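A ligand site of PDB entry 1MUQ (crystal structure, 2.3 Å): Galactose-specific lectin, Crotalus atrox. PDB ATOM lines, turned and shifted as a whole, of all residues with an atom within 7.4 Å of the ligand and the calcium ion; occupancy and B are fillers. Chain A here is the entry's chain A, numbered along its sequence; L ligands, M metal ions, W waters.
The side-chain carboxylate (OD2) of Asp 120 is in hydrogen-bond range of the backbone NH (N) of His 99. The backbone NH (N) of Glu 108 sits at hydrogen-bond distance from the backbone carbonyl oxygen (O) of Asn 119, 3.0 Å away. OE1 of Glu 104 sits close to OE1 of Gln 121, at 3.1 Å. OD1 of Asp 98 lies close to N of Tyr 100. The side-chain hydroxyl (OH) of Tyr 100 sits close to the side-chain amide nitrogen (NE2) of Gln 101, 3.2 Å away. OE1 of Glu 108 lies within hydrogen-bond range of NE2 of Gln 121, 3.0 Å away. The backbone NH (N) of Gln 121 is in hydrogen-bond range of the backbone carbonyl oxygen (O) of Cys 106, at 2.4 Å.
Merely in contact with the ligand: Tyr 100 (3.8 Å) and Gln 121 (3.9 Å). Seven residues have an atom within 4 Å of the ligand: Gln 96, Asp 98, Tyr 100, Glu 104, Asn 119, Asp 120 and Gln 121.
Within 4 Å of the calcium ion: Gln 96, Asp 98, Glu 104, Asn 119 and Asp 120. The nearest printed residue that does not touch the calcium ion is Tyr 100 (4.6 Å).
OD1 of Asp 120 is bound to the calcium ion, 2.2 Å away. OD1 of Asn 119 binds the calcium ion (2.3 Å). The calcium ion is bound by the side-chain amide oxygen (OE1) of Gln 96 (2.4 Å). OE2 of Glu 104 is bound to the calcium ion. O of Asp 120 is bound to the calcium ion (2.5 Å). The calcium ion is bound by OD1 of Asp 98 (2.5 Å). O4 of the ligand binds the calcium ion, at 2.7 Å. An oxygen (O3) of the ligand is bound to the calcium ion (2.8 Å). The calcium ion has eight donor atoms within binding distance.
Water W1 lies within hydrogen-bond range of O2 of the ligand (2.8 Å) and ND2 of Asn 119 (3.5 Å).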
ATOM      1  N   ASN A  65      15.509   9.274  37.042  1.00  0.00           N
ATOM      2  CA  ASN A  65      15.560  10.623  36.536  1.00  0.00           C
ATOM      3  C   ASN A  65      15.250  11.561  37.711  1.00  0.00           C
ATOM      4  O   ASN A  65      14.748  11.112  38.756  1.00  0.00           O
ATOM      5  CB  ASN A  65      14.549  10.834  35.414  1.00  0.00           C
ATOM      6  CG  ASN A  65      14.826   9.935  34.226  1.00  0.00           C
ATOM      7  OD1 ASN A  65      15.979   9.673  33.872  1.00  0.00           O
ATOM      8  ND2 ASN A  65      13.761   9.464  33.589  1.00  0.00           N
ATOM      9  N   TRP A  92      16.425  20.881  26.480  1.00  0.00           N
ATOM     10  CA  TRP A  92      15.649  19.686  26.247  1.00  0.00           C
ATOM     11  C   TRP A  92      16.466  18.570  25.632  1.00  0.00           C
ATOM     12  O   TRP A  92      17.426  18.818  24.911  1.00  0.00           O
ATOM     13  CB  TRP A  92      14.474  19.983  25.309  1.00  0.00           C
ATOM     14  CG  TRP A  92      13.490  20.939  25.891  1.00  0.00           C
ATOM     15  CD1 TRP A  92      13.324  22.246  25.551  1.00  0.00           C
ATOM     16  CD2 TRP A  92      12.544  20.658  26.927  1.00  0.00           C
ATOM     17  NE1 TRP A  92      12.332  22.808  26.321  1.00  0.00           N
ATOM     18  CE2 TRP A  92      11.831  21.850  27.176  1.00  0.00           C
ATOM     19  CE3 TRP A  92      12.230  19.515  27.675  1.00  0.00           C
ATOM     20  CZ2 TRP A  92      10.829  21.935  28.130  1.00  0.00           C
ATOM     21  CZ3 TRP A  92      11.233  19.605  28.622  1.00  0.00           C
ATOM     22  CH2 TRP A  92      10.534  20.806  28.844  1.00  0.00           C
ATOM     23  N   ASP A  93      16.084  17.337  25.943  1.00  0.00           N
ATOM     24  CA  ASP A  93      16.761  16.174  25.403  1.00  0.00           C
ATOM     25  C   ASP A  93      16.279  16.003  23.972  1.00  0.00           C
ATOM     26  O   ASP A  93      15.332  16.671  23.545  1.00  0.00           O
ATOM     27  CB  ASP A  93      16.415  14.941  26.221  1.00  0.00           C
ATOM     28  CG  ASP A  93      17.288  13.757  25.870  1.00  0.00           C
ATOM     29  OD1 ASP A  93      18.229  13.935  25.065  1.00  0.00           O
ATOM     30  OD2 ASP A  93      17.020  12.657  26.403  1.00  0.00           O
ATOM     31  N   LYS A  94      16.922  15.110  23.236  1.00  0.00           N
ATOM     32  CA  LYS A  94      16.543  14.871  21.852  1.00  0.00           C
ATOM     33  C   LYS A  94      15.080  14.469  21.750  1.00  0.00           C
ATOM     34  O   LYS A  94      14.631  13.556  22.458  1.00  0.00           O
ATOM     35  CB  LYS A  94      17.433  13.765  21.260  1.00  0.00           C
ATOM     36  CG  LYS A  94      17.263  13.563  19.760  1.00  0.00           C
ATOM     37  CD  LYS A  94      18.188  12.459  19.257  1.00  0.00           C
ATOM     38  CE  LYS A  94      18.037  12.236  17.771  1.00  0.00           C
ATOM     39  NZ  LYS A  94      18.889  11.110  17.297  1.00  0.00           N
ATOM     40  N   ASN A  95      14.334  15.160  20.892  1.00  0.00           N
ATOM     41  CA  ASN A  95      12.922  14.887  20.660  1.00  0.00           C
ATOM     42  C   ASN A  95      12.004  15.309  21.803  1.00  0.00           C
ATOM     43  O   ASN A  95      10.900  14.780  21.940  1.00  0.00           O
ATOM     44  CB  ASN A  95      12.726  13.396  20.404  1.00  0.00           C
ATOM     45  CG  ASN A  95      13.430  12.921  19.167  1.00  0.00           C
ATOM     46  OD1 ASN A  95      13.680  11.721  19.000  1.00  0.00           O
ATOM     47  ND2 ASN A  95      13.772  13.847  18.279  1.00  0.00           N
ATOM     48  N   GLN A  96      12.448  16.258  22.612  1.00  0.00           N
ATOM     49  CA  GLN A  96      11.639  16.720  23.724  1.00  0.00           C
ATOM     50  C   GLN A  96      11.562  18.242  23.662  1.00  0.00           C
ATOM     51  O   GLN A  96      12.397  18.871  23.023  1.00  0.00           O
ATOM     52  CB  GLN A  96      12.264  16.280  25.048  1.00  0.00           C
ATOM     53  CG  GLN A  96      12.585  14.794  25.155  1.00  0.00           C
ATOM     54  CD  GLN A  96      11.360  13.901  25.128  1.00  0.00           C
ATOM     55  OE1 GLN A  96      10.238  14.356  25.354  1.00  0.00           O
ATOM     56  NE2 GLN A  96      11.570  12.611  24.861  1.00  0.00           N
ATOM     57  N   PRO A  97      10.559  18.855  24.299  1.00  0.00           N
ATOM     58  CA  PRO A  97       9.471  18.218  25.055  1.00  0.00           C
ATOM     59  C   PRO A  97       8.433  17.739  24.045  1.00  0.00           C
ATOM     60  O   PRO A  97       8.208  18.393  23.028  1.00  0.00           O
ATOM     61  CB  PRO A  97       8.969  19.354  25.924  1.00  0.00           C
ATOM     62  CG  PRO A  97       9.077  20.532  25.006  1.00  0.00           C
ATOM     63  CD  PRO A  97      10.437  20.320  24.337  1.00  0.00           C
ATOM     64  N   ASP A  98       7.806  16.605  24.322  1.00  0.00           N
ATOM     65  CA  ASP A  98       6.832  16.084  23.376  1.00  0.00           C
ATOM     66  C   ASP A  98       5.416  15.865  23.884  1.00  0.00           C
ATOM     67  O   ASP A  98       4.581  15.367  23.129  1.00  0.00           O
ATOM     68  CB  ASP A  98       7.327  14.770  22.784  1.00  0.00           C
ATOM     69  CG  ASP A  98       7.564  13.712  23.833  1.00  0.00           C
ATOM     70  OD1 ASP A  98       7.184  13.930  25.004  1.00  0.00           O
ATOM     71  OD2 ASP A  98       8.126  12.661  23.494  1.00  0.00           O
ATOM     72  N   HIS A  99       5.135  16.236  25.131  1.00  0.00           N
ATOM     73  CA  HIS A  99       3.800  16.031  25.685  1.00  0.00           C
ATOM     74  C   HIS A  99       3.308  14.642  25.251  1.00  0.00           C
ATOM     75  O   HIS A  99       2.182  14.493  24.764  1.00  0.00           O
ATOM     76  CB  HIS A  99       2.835  17.100  25.159  1.00  0.00           C
ATOM     77  CG  HIS A  99       2.929  18.411  25.868  1.00  0.00           C
ATOM     78  ND1 HIS A  99       2.070  19.455  25.619  1.00  0.00           N
ATOM     79  CD2 HIS A  99       3.772  18.839  26.846  1.00  0.00           C
ATOM     80  CE1 HIS A  99       2.377  20.468  26.409  1.00  0.00           C
ATOM     81  NE2 HIS A  99       3.407  20.126  27.165  1.00  0.00           N
ATOM     82  N   TYR A 100       4.165  13.650  25.420  1.00  0.00           N
ATOM     83  CA  TYR A 100       3.836  12.289  25.036  1.00  0.00           C
ATOM     84  C   TYR A 100       2.426  11.891  25.472  1.00  0.00           C
ATOM     85  O   TYR A 100       2.102  11.888  26.671  1.00  0.00           O
ATOM     86  CB  TYR A 100       4.862  11.331  25.635  1.00  0.00           C
ATOM     87  CG  TYR A 100       4.742   9.915  25.139  1.00  0.00           C
ATOM     88  CD1 TYR A 100       4.644   8.856  26.036  1.00  0.00           C
ATOM     89  CD2 TYR A 100       4.751   9.636  23.771  1.00  0.00           C
ATOM     90  CE1 TYR A 100       4.554   7.545  25.584  1.00  0.00           C
ATOM     91  CE2 TYR A 100       4.667   8.330  23.312  1.00  0.00           C
ATOM     92  CZ  TYR A 100       4.574   7.286  24.224  1.00  0.00           C
ATOM     93  OH  TYR A 100       4.507   5.985  23.798  1.00  0.00           O
ATOM     94  N   GLN A 101       1.596  11.572  24.483  1.00  0.00           N
ATOM     95  CA  GLN A 101       0.209  11.172  24.728  1.00  0.00           C
ATOM     96  C   GLN A 101      -0.590  12.206  25.505  1.00  0.00           C
ATOM     97  O   GLN A 101      -1.590  11.876  26.146  1.00  0.00           O
ATOM     98  CB  GLN A 101       0.177   9.823  25.444  1.00  0.00           C
ATOM     99  CG  GLN A 101       0.646   8.658  24.585  1.00  0.00           C
ATOM    100  CD  GLN A 101       0.634   7.338  25.339  1.00  0.00           C
ATOM    101  OE1 GLN A 101      -0.345   7.011  26.000  1.00  0.00           O
ATOM    102  NE2 GLN A 101       1.719   6.576  25.224  1.00  0.00           N
ATOM    103  N   GLU A 104       2.307  14.364  29.635  1.00  0.00           N
ATOM    104  CA  GLU A 104       3.573  14.782  30.231  1.00  0.00           C
ATOM    105  C   GLU A 104       3.684  16.315  30.256  1.00  0.00           C
ATOM    106  O   GLU A 104       3.728  16.966  29.201  1.00  0.00           O
ATOM    107  CB  GLU A 104       4.731  14.165  29.448  1.00  0.00           C
ATOM    108  CG  GLU A 104       4.773  12.639  29.538  1.00  0.00           C
ATOM    109  CD  GLU A 104       5.940  12.015  28.788  1.00  0.00           C
ATOM    110  OE1 GLU A 104       6.301  10.852  29.082  1.00  0.00           O
ATOM    111  OE2 GLU A 104       6.481  12.688  27.884  1.00  0.00           O
ATOM    112  N   CYS A 106       5.531  17.744  33.252  1.00  0.00           N
ATOM    113  CA  CYS A 106       6.514  17.989  34.309  1.00  0.00           C
ATOM    114  C   CYS A 106       7.882  17.575  33.821  1.00  0.00           C
ATOM    115  O   CYS A 106       8.052  16.512  33.215  1.00  0.00           O
ATOM    116  CB  CYS A 106       6.118  17.224  35.574  1.00  0.00           C
ATOM    117  SG  CYS A 106       4.644  17.918  36.382  1.00  0.00           S
ATOM    118  N   GLU A 108      11.929  16.592  34.030  1.00  0.00           N
ATOM    119  CA  GLU A 108      12.892  15.830  34.802  1.00  0.00           C
ATOM    120  C   GLU A 108      14.249  15.840  34.088  1.00  0.00           C
ATOM    121  O   GLU A 108      14.327  16.027  32.874  1.00  0.00           O
ATOM    122  CB  GLU A 108      12.416  14.385  34.935  1.00  0.00           C
ATOM    123  CG  GLU A 108      12.461  13.612  33.611  1.00  0.00           C
ATOM    124  CD  GLU A 108      11.829  12.242  33.690  1.00  0.00           C
ATOM    125  OE1 GLU A 108      11.907  11.491  32.693  1.00  0.00           O
ATOM    126  OE2 GLU A 108      11.241  11.908  34.737  1.00  0.00           O
ATOM    127  N   VAL A 110      17.141  13.837  32.634  1.00  0.00           N
ATOM    128  CA  VAL A 110      17.263  12.475  32.150  1.00  0.00           C
ATOM    129  C   VAL A 110      18.578  11.823  32.545  1.00  0.00           C
ATOM    130  O   VAL A 110      19.672  12.296  32.207  1.00  0.00           O
ATOM    131  CB  VAL A 110      17.086  12.438  30.620  1.00  0.00           C
ATOM    132  CG1 VAL A 110      17.151  11.003  30.125  1.00  0.00           C
ATOM    133  CG2 VAL A 110      15.753  13.050  30.241  1.00  0.00           C
ATOM    134  N   LEU A 112      19.937   9.073  31.507  1.00  0.00           N
ATOM    135  CA  LEU A 112      20.739   8.565  30.400  1.00  0.00           C
ATOM    136  C   LEU A 112      21.638   9.624  29.779  1.00  0.00           C
ATOM    137  O   LEU A 112      22.635   9.283  29.135  1.00  0.00           O
ATOM    138  CB  LEU A 112      19.836   7.967  29.305  1.00  0.00           C
ATOM    139  CG  LEU A 112      19.175   6.620  29.602  1.00  0.00           C
ATOM    140  CD1 LEU A 112      18.340   6.191  28.406  1.00  0.00           C
ATOM    141  CD2 LEU A 112      20.257   5.582  29.903  1.00  0.00           C
ATOM    142  N   TRP A 118      16.846  17.675  29.579  1.00  0.00           N
ATOM    143  CA  TRP A 118      15.497  17.580  30.130  1.00  0.00           C
ATOM    144  C   TRP A 118      14.494  16.831  29.273  1.00  0.00           C
ATOM    145  O   TRP A 118      14.606  16.778  28.039  1.00  0.00           O
ATOM    146  CB  TRP A 118      14.910  18.969  30.346  1.00  0.00           C
ATOM    147  CG  TRP A 118      15.808  19.941  31.018  1.00  0.00           C
ATOM    148  CD1 TRP A 118      16.919  19.665  31.769  1.00  0.00           C
ATOM    149  CD2 TRP A 118      15.632  21.357  31.050  1.00  0.00           C
ATOM    150  NE1 TRP A 118      17.443  20.830  32.269  1.00  0.00           N
ATOM    151  CE2 TRP A 118      16.681  21.884  31.851  1.00  0.00           C
ATOM    152  CE3 TRP A 118      14.695  22.231  30.503  1.00  0.00           C
ATOM    153  CZ2 TRP A 118      16.811  23.249  32.093  1.00  0.00           C
ATOM    154  CZ3 TRP A 118      14.823  23.590  30.739  1.00  0.00           C
ATOM    155  CH2 TRP A 118      15.877  24.081  31.531  1.00  0.00           C
ATOM    156  N   ASN A 119      13.486  16.295  29.947  1.00  0.00           N
ATOM    157  CA  ASN A 119      12.417  15.576  29.282  1.00  0.00           C
ATOM    158  C   ASN A 119      11.097  15.862  30.011  1.00  0.00           C
ATOM    159  O   ASN A 119      11.055  15.811  31.238  1.00  0.00           O
ATOM    160  CB  ASN A 119      12.672  14.075  29.295  1.00  0.00           C
ATOM    161  CG  ASN A 119      11.445  13.275  28.919  1.00  0.00           C
ATOM    162  OD1 ASN A 119      10.838  13.503  27.883  1.00  0.00           O
ATOM    163  ND2 ASN A 119      11.056  12.337  29.776  1.00  0.00           N
ATOM    164  N   ASP A 120      10.041  16.170  29.268  1.00  0.00           N
ATOM    165  CA  ASP A 120       8.762  16.398  29.911  1.00  0.00           C
ATOM    166  C   ASP A 120       8.296  14.991  30.247  1.00  0.00           C
ATOM    167  O   ASP A 120       8.399  14.069  29.439  1.00  0.00           O
ATOM    168  CB  ASP A 120       7.790  17.127  28.988  1.00  0.00           C
ATOM    169  CG  ASP A 120       7.684  16.502  27.623  1.00  0.00           C
ATOM    170  OD1 ASP A 120       8.575  15.702  27.263  1.00  0.00           O
ATOM    171  OD2 ASP A 120       6.712  16.823  26.913  1.00  0.00           O
ATOM    172  N   GLN A 121       7.806  14.817  31.465  1.00  0.00           N
ATOM    173  CA  GLN A 121       7.412  13.521  31.957  1.00  0.00           C
ATOM    174  C   GLN A 121       6.033  13.577  32.599  1.00  0.00           C
ATOM    175  O   GLN A 121       5.542  14.658  32.973  1.00  0.00           O
ATOM    176  CB  GLN A 121       8.467  13.090  32.994  1.00  0.00           C
ATOM    177  CG  GLN A 121       8.313  11.713  33.575  1.00  0.00           C
ATOM    178  CD  GLN A 121       8.151  10.672  32.507  1.00  0.00           C
ATOM    179  OE1 GLN A 121       7.028  10.369  32.084  1.00  0.00           O
ATOM    180  NE2 GLN A 121       9.276  10.136  32.029  1.00  0.00           N
ATOM    181  N   VAL A 122       5.414  12.410  32.706  1.00  0.00           N
ATOM    182  CA  VAL A 122       4.110  12.292  33.337  1.00  0.00           C
ATOM    183  C   VAL A 122       4.344  12.783  34.764  1.00  0.00           C
ATOM    184  O   VAL A 122       5.202  12.249  35.474  1.00  0.00           O
ATOM    185  CB  VAL A 122       3.640  10.829  33.342  1.00  0.00           C
ATOM    186  CG1 VAL A 122       2.461  10.683  34.262  1.00  0.00           C
ATOM    187  CG2 VAL A 122       3.311  10.382  31.917  1.00  0.00           C
HETATM  188  C1  LIG L   1      11.165   8.805  26.312  1.00  0.00           C
HETATM  189  C2  LIG L   1      10.646   9.813  27.356  1.00  0.00           C
HETATM  190  C3  LIG L   1       9.108   9.825  27.402  1.00  0.00           C
HETATM  191  C4  LIG L   1       8.495   9.905  26.009  1.00  0.00           C
HETATM  192  C5  LIG L   1       9.133   8.885  25.069  1.00  0.00           C
HETATM  193  C6  LIG L   1       8.637   8.966  23.653  1.00  0.00           C
HETATM  194  O1  LIG L   1      12.544   8.922  26.175  1.00  0.00           O
HETATM  195  O2  LIG L   1      11.147   9.463  28.632  1.00  0.00           O
HETATM  196  O3  LIG L   1       8.691  10.951  28.139  1.00  0.00           O
HETATM  197  O4  LIG L   1       8.675  11.221  25.494  1.00  0.00           O
HETATM  198  O5  LIG L   1      10.560   9.071  25.037  1.00  0.00           O
HETATM  199  O6  LIG L   1       8.406   7.664  23.122  1.00  0.00           O
HETATM  200 CA    CA M   1       8.683  13.511  26.993  1.00  0.00          CA
HETATM  201  O   HOH W   1      13.745  10.571  28.471  1.00  0.00           O
HETATM  202  O   HOH W   2      11.072   8.313  22.356  1.00  0.00           O
